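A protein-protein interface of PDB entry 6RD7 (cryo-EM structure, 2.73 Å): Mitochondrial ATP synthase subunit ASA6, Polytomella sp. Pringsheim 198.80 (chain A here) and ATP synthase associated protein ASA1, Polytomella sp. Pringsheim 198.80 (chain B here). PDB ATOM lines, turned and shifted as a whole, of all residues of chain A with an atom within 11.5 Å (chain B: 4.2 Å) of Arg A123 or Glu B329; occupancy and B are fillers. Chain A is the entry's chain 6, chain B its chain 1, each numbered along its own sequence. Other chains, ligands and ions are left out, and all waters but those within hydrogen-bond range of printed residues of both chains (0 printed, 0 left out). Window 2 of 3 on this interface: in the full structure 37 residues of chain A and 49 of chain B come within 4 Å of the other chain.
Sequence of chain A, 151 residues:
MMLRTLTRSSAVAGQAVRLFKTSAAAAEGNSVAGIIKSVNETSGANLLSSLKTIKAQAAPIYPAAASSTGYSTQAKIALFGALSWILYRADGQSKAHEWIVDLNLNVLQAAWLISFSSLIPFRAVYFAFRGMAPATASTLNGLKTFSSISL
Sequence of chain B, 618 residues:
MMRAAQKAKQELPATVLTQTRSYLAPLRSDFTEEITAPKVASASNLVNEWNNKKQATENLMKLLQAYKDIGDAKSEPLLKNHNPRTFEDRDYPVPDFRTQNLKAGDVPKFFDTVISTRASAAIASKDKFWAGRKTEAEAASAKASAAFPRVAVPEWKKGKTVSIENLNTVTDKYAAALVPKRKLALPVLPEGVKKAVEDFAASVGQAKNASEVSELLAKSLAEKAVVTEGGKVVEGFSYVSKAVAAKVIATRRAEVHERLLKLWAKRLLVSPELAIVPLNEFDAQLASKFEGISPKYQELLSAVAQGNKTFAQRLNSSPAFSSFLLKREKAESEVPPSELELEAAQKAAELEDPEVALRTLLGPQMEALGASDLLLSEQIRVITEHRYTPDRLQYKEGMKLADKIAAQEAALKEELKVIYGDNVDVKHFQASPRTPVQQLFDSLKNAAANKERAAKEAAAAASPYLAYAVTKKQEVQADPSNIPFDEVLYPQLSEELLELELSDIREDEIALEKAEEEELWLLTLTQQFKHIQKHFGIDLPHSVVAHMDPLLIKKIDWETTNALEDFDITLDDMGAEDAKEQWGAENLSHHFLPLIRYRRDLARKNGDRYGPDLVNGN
OE1 of Glu B334 is in salt-bridge range of NE of Arg A123. The guanidinium group of Arg A123 lies within salt-bridge range of the side-chain carboxylate of Glu B329 (2.9 Å).
The side-chain hydroxyl (OH) of Tyr A126 is in hydrogen-bond range of the guanidinium group (NH2) of Arg A130 (3.4 Å).
Among the printed residues, merely in contact across the chains: Arg A123 with Lys B330, Phe A127 with Glu B334, Arg A123 with Leu B326, Phe A127 with Phe B321, Phe A122 with Leu B326, Arg A123 with Ser B333, Tyr A126 with Phe B321 and Ala A124 with Glu B334.
Of the printed residues of chain B, Phe A122 touches Leu B326 (3.8 Å). Of the printed residues of chain B, Arg A123 touches Leu B326, Glu B329, Lys B330, Ser B333 and Glu B334. Printed residues of chain B within 4 Å of Ala A124: Glu B334 (3.9 Å). Val A125 touches none of the printed residues of chain B. Of the printed residues of chain B, Tyr A126 touches Phe B321. Gly A131 touches none of the printed residues of chain B. Phe B321 touches two residues of chain A. Of chain A, only Phe A122 and Arg A123 come within 4 Å of Leu B326. Of chain A, only Arg A123 (3.4 Å) comes within 4 Å of Lys B330. Ser B333 touches one residue of chain A. The nearest residue of chain A that does not touch Glu B329 is Phe A122 (5.6 Å).
Printed residues of chain A that touch a printed residue of chain B: Phe A122, Arg A123, Ala A124, Tyr A126 and Phe A127. Of the 8 printed residues of chain B, 6 touch a printed residue of chain A. Printed residues of chain B that touch a printed residue of chain A: Phe B321, Leu B326, Glu B329, Lys B330, Ser B333 and Glu B334. Among the printed residues, 10 pairs touch across the chains. Among the printed residues, Asp or Glu carboxylates within 4 Å of a Lys or Arg side-chain nitrogen of the other chain: Arg A123 with Glu B329 and Arg A123 with Glu B334.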
ATOM      1  N   PHE A 116       9.870  25.751  26.669  1.00  0.00           N
ATOM      2  CA  PHE A 116      10.174  25.093  25.401  1.00  0.00           C
ATOM      3  C   PHE A 116       8.928  24.888  24.568  1.00  0.00           C
ATOM      4  O   PHE A 116       8.988  24.927  23.337  1.00  0.00           O
ATOM      5  CB  PHE A 116      10.832  23.744  25.650  1.00  0.00           C
ATOM      6  CG  PHE A 116      12.263  23.832  26.030  1.00  0.00           C
ATOM      7  CD1 PHE A 116      13.033  24.923  25.664  1.00  0.00           C
ATOM      8  CD2 PHE A 116      12.833  22.841  26.795  1.00  0.00           C
ATOM      9  CE1 PHE A 116      14.364  24.994  26.028  1.00  0.00           C
ATOM     10  CE2 PHE A 116      14.145  22.923  27.164  1.00  0.00           C
ATOM     11  CZ  PHE A 116      14.919  23.994  26.789  1.00  0.00           C
ATOM     12  N   SER A 117       7.795  24.634  25.224  1.00  0.00           N
ATOM     13  CA  SER A 117       6.537  24.507  24.493  1.00  0.00           C
ATOM     14  C   SER A 117       6.125  25.831  23.852  1.00  0.00           C
ATOM     15  O   SER A 117       5.412  25.851  22.844  1.00  0.00           O
ATOM     16  CB  SER A 117       5.448  24.001  25.431  1.00  0.00           C
ATOM     17  OG  SER A 117       5.703  22.661  25.806  1.00  0.00           O
ATOM     18  N   SER A 118       6.583  26.948  24.417  1.00  0.00           N
ATOM     19  CA  SER A 118       6.176  28.259  23.929  1.00  0.00           C
ATOM     20  C   SER A 118       7.158  28.799  22.897  1.00  0.00           C
ATOM     21  O   SER A 118       6.757  29.447  21.923  1.00  0.00           O
ATOM     22  CB  SER A 118       6.057  29.224  25.107  1.00  0.00           C
ATOM     23  OG  SER A 118       4.937  28.913  25.911  1.00  0.00           O
ATOM     24  N   LEU A 119       8.452  28.542  23.091  1.00  0.00           N
ATOM     25  CA  LEU A 119       9.467  29.281  22.347  1.00  0.00           C
ATOM     26  C   LEU A 119       9.860  28.582  21.053  1.00  0.00           C
ATOM     27  O   LEU A 119      10.268  29.241  20.090  1.00  0.00           O
ATOM     28  CB  LEU A 119      10.699  29.493  23.222  1.00  0.00           C
ATOM     29  CG  LEU A 119      10.589  30.522  24.345  1.00  0.00           C
ATOM     30  CD1 LEU A 119      11.892  30.583  25.124  1.00  0.00           C
ATOM     31  CD2 LEU A 119      10.220  31.887  23.794  1.00  0.00           C
ATOM     32  N   ILE A 120       9.761  27.260  21.006  1.00  0.00           N
ATOM     33  CA  ILE A 120      10.369  26.510  19.900  1.00  0.00           C
ATOM     34  C   ILE A 120       9.483  26.608  18.661  1.00  0.00           C
ATOM     35  O   ILE A 120       8.289  26.272  18.728  1.00  0.00           O
ATOM     36  CB  ILE A 120      10.592  25.054  20.304  1.00  0.00           C
ATOM     37  CG1 ILE A 120      11.695  24.956  21.351  1.00  0.00           C
ATOM     38  CG2 ILE A 120      10.986  24.225  19.107  1.00  0.00           C
ATOM     39  CD1 ILE A 120      11.876  23.565  21.901  1.00  0.00           C
ATOM     40  N   PRO A 121      10.013  27.064  17.522  1.00  0.00           N
ATOM     41  CA  PRO A 121       9.233  27.063  16.277  1.00  0.00           C
ATOM     42  C   PRO A 121       9.141  25.675  15.661  1.00  0.00           C
ATOM     43  O   PRO A 121       9.997  25.296  14.857  1.00  0.00           O
ATOM     44  CB  PRO A 121      10.003  28.038  15.379  1.00  0.00           C
ATOM     45  CG  PRO A 121      11.395  28.036  15.902  1.00  0.00           C
ATOM     46  CD  PRO A 121      11.368  27.610  17.338  1.00  0.00           C
ATOM     47  N   PHE A 122       8.119  24.909  16.062  1.00  0.00           N
ATOM     48  CA  PHE A 122       8.073  23.474  15.785  1.00  0.00           C
ATOM     49  C   PHE A 122       7.968  23.164  14.295  1.00  0.00           C
ATOM     50  O   PHE A 122       8.448  22.118  13.843  1.00  0.00           O
ATOM     51  CB  PHE A 122       6.910  22.845  16.544  1.00  0.00           C
ATOM     52  CG  PHE A 122       7.157  22.708  18.012  1.00  0.00           C
ATOM     53  CD1 PHE A 122       8.177  21.898  18.481  1.00  0.00           C
ATOM     54  CD2 PHE A 122       6.381  23.396  18.925  1.00  0.00           C
ATOM     55  CE1 PHE A 122       8.410  21.772  19.833  1.00  0.00           C
ATOM     56  CE2 PHE A 122       6.611  23.273  20.278  1.00  0.00           C
ATOM     57  CZ  PHE A 122       7.627  22.461  20.730  1.00  0.00           C
ATOM     58  N   ARG A 123       7.369  24.061  13.511  1.00  0.00           N
ATOM     59  CA  ARG A 123       7.326  23.852  12.068  1.00  0.00           C
ATOM     60  C   ARG A 123       8.698  24.054  11.442  1.00  0.00           C
ATOM     61  O   ARG A 123       9.114  23.279  10.570  1.00  0.00           O
ATOM     62  CB  ARG A 123       6.304  24.786  11.431  1.00  0.00           C
ATOM     63  CG  ARG A 123       5.908  24.395  10.027  1.00  0.00           C
ATOM     64  CD  ARG A 123       5.416  25.592   9.246  1.00  0.00           C
ATOM     65  NE  ARG A 123       6.400  26.666   9.228  1.00  0.00           N
ATOM     66  CZ  ARG A 123       6.180  27.883   9.708  1.00  0.00           C
ATOM     67  NH1 ARG A 123       5.009  28.181  10.249  1.00  0.00           N
ATOM     68  NH2 ARG A 123       7.132  28.802   9.650  1.00  0.00           N
ATOM     69  N   ALA A 124       9.423  25.079  11.891  1.00  0.00           N
ATOM     70  CA  ALA A 124      10.780  25.301  11.411  1.00  0.00           C
ATOM     71  C   ALA A 124      11.714  24.192  11.869  1.00  0.00           C
ATOM     72  O   ALA A 124      12.626  23.804  11.136  1.00  0.00           O
ATOM     73  CB  ALA A 124      11.286  26.660  11.885  1.00  0.00           C
ATOM     74  N   VAL A 125      11.471  23.639  13.058  1.00  0.00           N
ATOM     75  CA  VAL A 125      12.279  22.529  13.556  1.00  0.00           C
ATOM     76  C   VAL A 125      12.002  21.263  12.752  1.00  0.00           C
ATOM     77  O   VAL A 125      12.929  20.519  12.406  1.00  0.00           O
ATOM     78  CB  VAL A 125      12.022  22.337  15.063  1.00  0.00           C
ATOM     79  CG1 VAL A 125      12.574  21.017  15.568  1.00  0.00           C
ATOM     80  CG2 VAL A 125      12.640  23.478  15.833  1.00  0.00           C
ATOM     81  N   TYR A 126      10.731  21.023  12.407  1.00  0.00           N
ATOM     82  CA  TYR A 126      10.370  19.881  11.568  1.00  0.00           C
ATOM     83  C   TYR A 126      11.004  19.981  10.186  1.00  0.00           C
ATOM     84  O   TYR A 126      11.577  19.005   9.683  1.00  0.00           O
ATOM     85  CB  TYR A 126       8.847  19.784  11.447  1.00  0.00           C
ATOM     86  CG  TYR A 126       8.366  18.722  10.482  1.00  0.00           C
ATOM     87  CD1 TYR A 126       8.345  17.387  10.851  1.00  0.00           C
ATOM     88  CD2 TYR A 126       7.930  19.055   9.204  1.00  0.00           C
ATOM     89  CE1 TYR A 126       7.919  16.413   9.978  1.00  0.00           C
ATOM     90  CE2 TYR A 126       7.508  18.086   8.322  1.00  0.00           C
ATOM     91  CZ  TYR A 126       7.502  16.768   8.717  1.00  0.00           C
ATOM     92  OH  TYR A 126       7.072  15.794   7.852  1.00  0.00           O
ATOM     93  N   PHE A 127      10.940  21.158   9.570  1.00  0.00           N
ATOM     94  CA  PHE A 127      11.486  21.292   8.225  1.00  0.00           C
ATOM     95  C   PHE A 127      13.006  21.390   8.242  1.00  0.00           C
ATOM     96  O   PHE A 127      13.658  21.130   7.226  1.00  0.00           O
ATOM     97  CB  PHE A 127      10.861  22.493   7.527  1.00  0.00           C
ATOM     98  CG  PHE A 127       9.536  22.192   6.910  1.00  0.00           C
ATOM     99  CD1 PHE A 127       9.458  21.491   5.723  1.00  0.00           C
ATOM    100  CD2 PHE A 127       8.363  22.589   7.526  1.00  0.00           C
ATOM    101  CE1 PHE A 127       8.239  21.204   5.155  1.00  0.00           C
ATOM    102  CE2 PHE A 127       7.141  22.306   6.961  1.00  0.00           C
ATOM    103  CZ  PHE A 127       7.079  21.612   5.775  1.00  0.00           C
ATOM    104  N   ALA A 128      13.593  21.753   9.383  1.00  0.00           N
ATOM    105  CA  ALA A 128      15.045  21.716   9.504  1.00  0.00           C
ATOM    106  C   ALA A 128      15.533  20.294   9.701  1.00  0.00           C
ATOM    107  O   ALA A 128      16.628  19.937   9.257  1.00  0.00           O
ATOM    108  CB  ALA A 128      15.501  22.600  10.661  1.00  0.00           C
ATOM    109  N   PHE A 129      14.736  19.466  10.376  1.00  0.00           N
ATOM    110  CA  PHE A 129      15.097  18.061  10.508  1.00  0.00           C
ATOM    111  C   PHE A 129      14.900  17.332   9.189  1.00  0.00           C
ATOM    112  O   PHE A 129      15.620  16.374   8.895  1.00  0.00           O
ATOM    113  CB  PHE A 129      14.281  17.401  11.620  1.00  0.00           C
ATOM    114  CG  PHE A 129      14.805  17.660  13.011  1.00  0.00           C
ATOM    115  CD1 PHE A 129      15.831  18.561  13.242  1.00  0.00           C
ATOM    116  CD2 PHE A 129      14.262  16.997  14.092  1.00  0.00           C
ATOM    117  CE1 PHE A 129      16.298  18.792  14.515  1.00  0.00           C
ATOM    118  CE2 PHE A 129      14.724  17.225  15.369  1.00  0.00           C
ATOM    119  CZ  PHE A 129      15.744  18.122  15.579  1.00  0.00           C
ATOM    120  N   ARG A 130      13.951  17.793   8.369  1.00  0.00           N
ATOM    121  CA  ARG A 130      13.774  17.226   7.034  1.00  0.00           C
ATOM    122  C   ARG A 130      14.963  17.514   6.128  1.00  0.00           C
ATOM    123  O   ARG A 130      15.217  16.761   5.185  1.00  0.00           O
ATOM    124  CB  ARG A 130      12.495  17.765   6.398  1.00  0.00           C
ATOM    125  CG  ARG A 130      11.271  16.926   6.659  1.00  0.00           C
ATOM    126  CD  ARG A 130      10.083  17.428   5.868  1.00  0.00           C
ATOM    127  NE  ARG A 130      10.042  16.877   4.518  1.00  0.00           N
ATOM    128  CZ  ARG A 130       9.518  15.698   4.206  1.00  0.00           C
ATOM    129  NH1 ARG A 130       9.526  15.282   2.950  1.00  0.00           N
ATOM    130  NH2 ARG A 130       8.987  14.934   5.145  1.00  0.00           N
ATOM    131  N   GLY A 131      15.695  18.593   6.385  1.00  0.00           N
ATOM    132  CA  GLY A 131      16.889  18.892   5.625  1.00  0.00           C
ATOM    133  C   GLY A 131      18.139  18.175   6.069  1.00  0.00           C
ATOM    134  O   GLY A 131      19.157  18.242   5.379  1.00  0.00           O
ATOM    135  N   MET A 132      18.096  17.487   7.209  1.00  0.00           N
ATOM    136  CA  MET A 132      19.260  16.747   7.680  1.00  0.00           C
ATOM    137  C   MET A 132      19.434  15.450   6.908  1.00  0.00           C
ATOM    138  O   MET A 132      20.561  15.033   6.623  1.00  0.00           O
ATOM    139  CB  MET A 132      19.134  16.462   9.174  1.00  0.00           C
ATOM    140  CG  MET A 132      19.245  17.686  10.042  1.00  0.00           C
ATOM    141  SD  MET A 132      18.793  17.339  11.742  1.00  0.00           S
ATOM    142  CE  MET A 132      19.976  16.070  12.146  1.00  0.00           C
ATOM    143  N   PHE B 321       1.729  16.210  10.341  1.00  0.00           N
ATOM    144  CA  PHE B 321       0.957  17.424  10.560  1.00  0.00           C
ATOM    145  C   PHE B 321      -0.365  17.152  11.258  1.00  0.00           C
ATOM    146  O   PHE B 321      -1.156  18.081  11.440  1.00  0.00           O
ATOM    147  CB  PHE B 321       0.721  18.150   9.238  1.00  0.00           C
ATOM    148  CG  PHE B 321       1.846  19.054   8.848  1.00  0.00           C
ATOM    149  CD1 PHE B 321       1.913  20.346   9.327  1.00  0.00           C
ATOM    150  CD2 PHE B 321       2.852  18.603   8.019  1.00  0.00           C
ATOM    151  CE1 PHE B 321       2.958  21.172   8.975  1.00  0.00           C
ATOM    152  CE2 PHE B 321       3.896  19.423   7.663  1.00  0.00           C
ATOM    153  CZ  PHE B 321       3.950  20.707   8.143  1.00  0.00           C
ATOM    154  N   LEU B 326       2.056  20.249  15.577  1.00  0.00           N
ATOM    155  CA  LEU B 326       1.891  20.723  14.212  1.00  0.00           C
ATOM    156  C   LEU B 326       0.452  20.638  13.720  1.00  0.00           C
ATOM    157  O   LEU B 326       0.240  20.492  12.514  1.00  0.00           O
ATOM    158  CB  LEU B 326       2.810  19.929  13.283  1.00  0.00           C
ATOM    159  CG  LEU B 326       4.282  20.119  13.643  1.00  0.00           C
ATOM    160  CD1 LEU B 326       5.148  19.008  13.138  1.00  0.00           C
ATOM    161  CD2 LEU B 326       4.753  21.436  13.113  1.00  0.00           C
ATOM    162  N   LYS B 327      -0.533  20.720  14.616  1.00  0.00           N
ATOM    163  CA  LYS B 327      -1.933  20.684  14.200  1.00  0.00           C
ATOM    164  C   LYS B 327      -2.319  21.955  13.459  1.00  0.00           C
ATOM    165  O   LYS B 327      -3.042  21.913  12.459  1.00  0.00           O
ATOM    166  CB  LYS B 327      -2.845  20.490  15.411  1.00  0.00           C
ATOM    167  CG  LYS B 327      -2.737  19.146  16.075  1.00  0.00           C
ATOM    168  CD  LYS B 327      -3.679  19.013  17.246  1.00  0.00           C
ATOM    169  CE  LYS B 327      -4.981  18.388  16.809  1.00  0.00           C
ATOM    170  NZ  LYS B 327      -4.780  16.988  16.355  1.00  0.00           N
ATOM    171  N   ARG B 328      -1.848  23.098  13.941  1.00  0.00           N
ATOM    172  CA  ARG B 328      -2.232  24.386  13.386  1.00  0.00           C
ATOM    173  C   ARG B 328      -1.229  24.924  12.382  1.00  0.00           C
ATOM    174  O   ARG B 328      -1.471  25.982  11.794  1.00  0.00           O
ATOM    175  CB  ARG B 328      -2.428  25.403  14.509  1.00  0.00           C
ATOM    176  CG  ARG B 328      -3.823  25.403  15.089  1.00  0.00           C
ATOM    177  CD  ARG B 328      -3.917  24.449  16.249  1.00  0.00           C
ATOM    178  NE  ARG B 328      -5.079  24.715  17.087  1.00  0.00           N
ATOM    179  CZ  ARG B 328      -6.127  23.908  17.178  1.00  0.00           C
ATOM    180  NH1 ARG B 328      -6.157  22.780  16.483  1.00  0.00           N
ATOM    181  NH2 ARG B 328      -7.140  24.225  17.969  1.00  0.00           N
ATOM    182  N   GLU B 329      -0.115  24.237  12.174  1.00  0.00           N
ATOM    183  CA  GLU B 329       0.845  24.668  11.175  1.00  0.00           C
ATOM    184  C   GLU B 329       0.433  24.167   9.800  1.00  0.00           C
ATOM    185  O   GLU B 329      -0.312  23.194   9.665  1.00  0.00           O
ATOM    186  CB  GLU B 329       2.246  24.166  11.517  1.00  0.00           C
ATOM    187  CG  GLU B 329       2.749  24.624  12.869  1.00  0.00           C
ATOM    188  CD  GLU B 329       2.754  26.130  13.009  1.00  0.00           C
ATOM    189  OE1 GLU B 329       2.243  26.634  14.031  1.00  0.00           O
ATOM    190  OE2 GLU B 329       3.272  26.812  12.102  1.00  0.00           O
ATOM    191  N   LYS B 330       0.922  24.852   8.774  1.00  0.00           N
ATOM    192  CA  LYS B 330       0.668  24.492   7.389  1.00  0.00           C
ATOM    193  C   LYS B 330       2.000  24.323   6.680  1.00  0.00           C
ATOM    194  O   LYS B 330       2.962  25.034   6.984  1.00  0.00           O
ATOM    195  CB  LYS B 330      -0.182  25.554   6.692  1.00  0.00           C
ATOM    196  CG  LYS B 330      -1.645  25.519   7.084  1.00  0.00           C
ATOM    197  CD  LYS B 330      -2.276  24.195   6.706  1.00  0.00           C
ATOM    198  CE  LYS B 330      -3.497  23.904   7.555  1.00  0.00           C
ATOM    199  NZ  LYS B 330      -4.120  22.602   7.194  1.00  0.00           N
ATOM    200  N   SER B 333       3.376  27.325   4.591  1.00  0.00           N
ATOM    201  CA  SER B 333       3.969  28.477   5.262  1.00  0.00           C
ATOM    202  C   SER B 333       5.490  28.418   5.241  1.00  0.00           C
ATOM    203  O   SER B 333       6.156  29.459   5.274  1.00  0.00           O
ATOM    204  CB  SER B 333       3.459  28.565   6.696  1.00  0.00           C
ATOM    205  OG  SER B 333       2.048  28.661   6.718  1.00  0.00           O
ATOM    206  N   GLU B 334       6.063  27.215   5.198  1.00  0.00           N
ATOM    207  CA  GLU B 334       7.517  27.114   5.163  1.00  0.00           C
ATOM    208  C   GLU B 334       8.049  27.367   3.762  1.00  0.00           C
ATOM    209  O   GLU B 334       8.766  28.344   3.525  1.00  0.00           O
ATOM    210  CB  GLU B 334       7.966  25.746   5.667  1.00  0.00           C
ATOM    211  CG  GLU B 334       9.437  25.700   6.036  1.00  0.00           C
ATOM    212  CD  GLU B 334       9.721  26.299   7.403  1.00  0.00           C
ATOM    213  OE1 GLU B 334       8.766  26.516   8.178  1.00  0.00           O
ATOM    214  OE2 GLU B 334      10.906  26.556   7.704  1.00  0.00           O
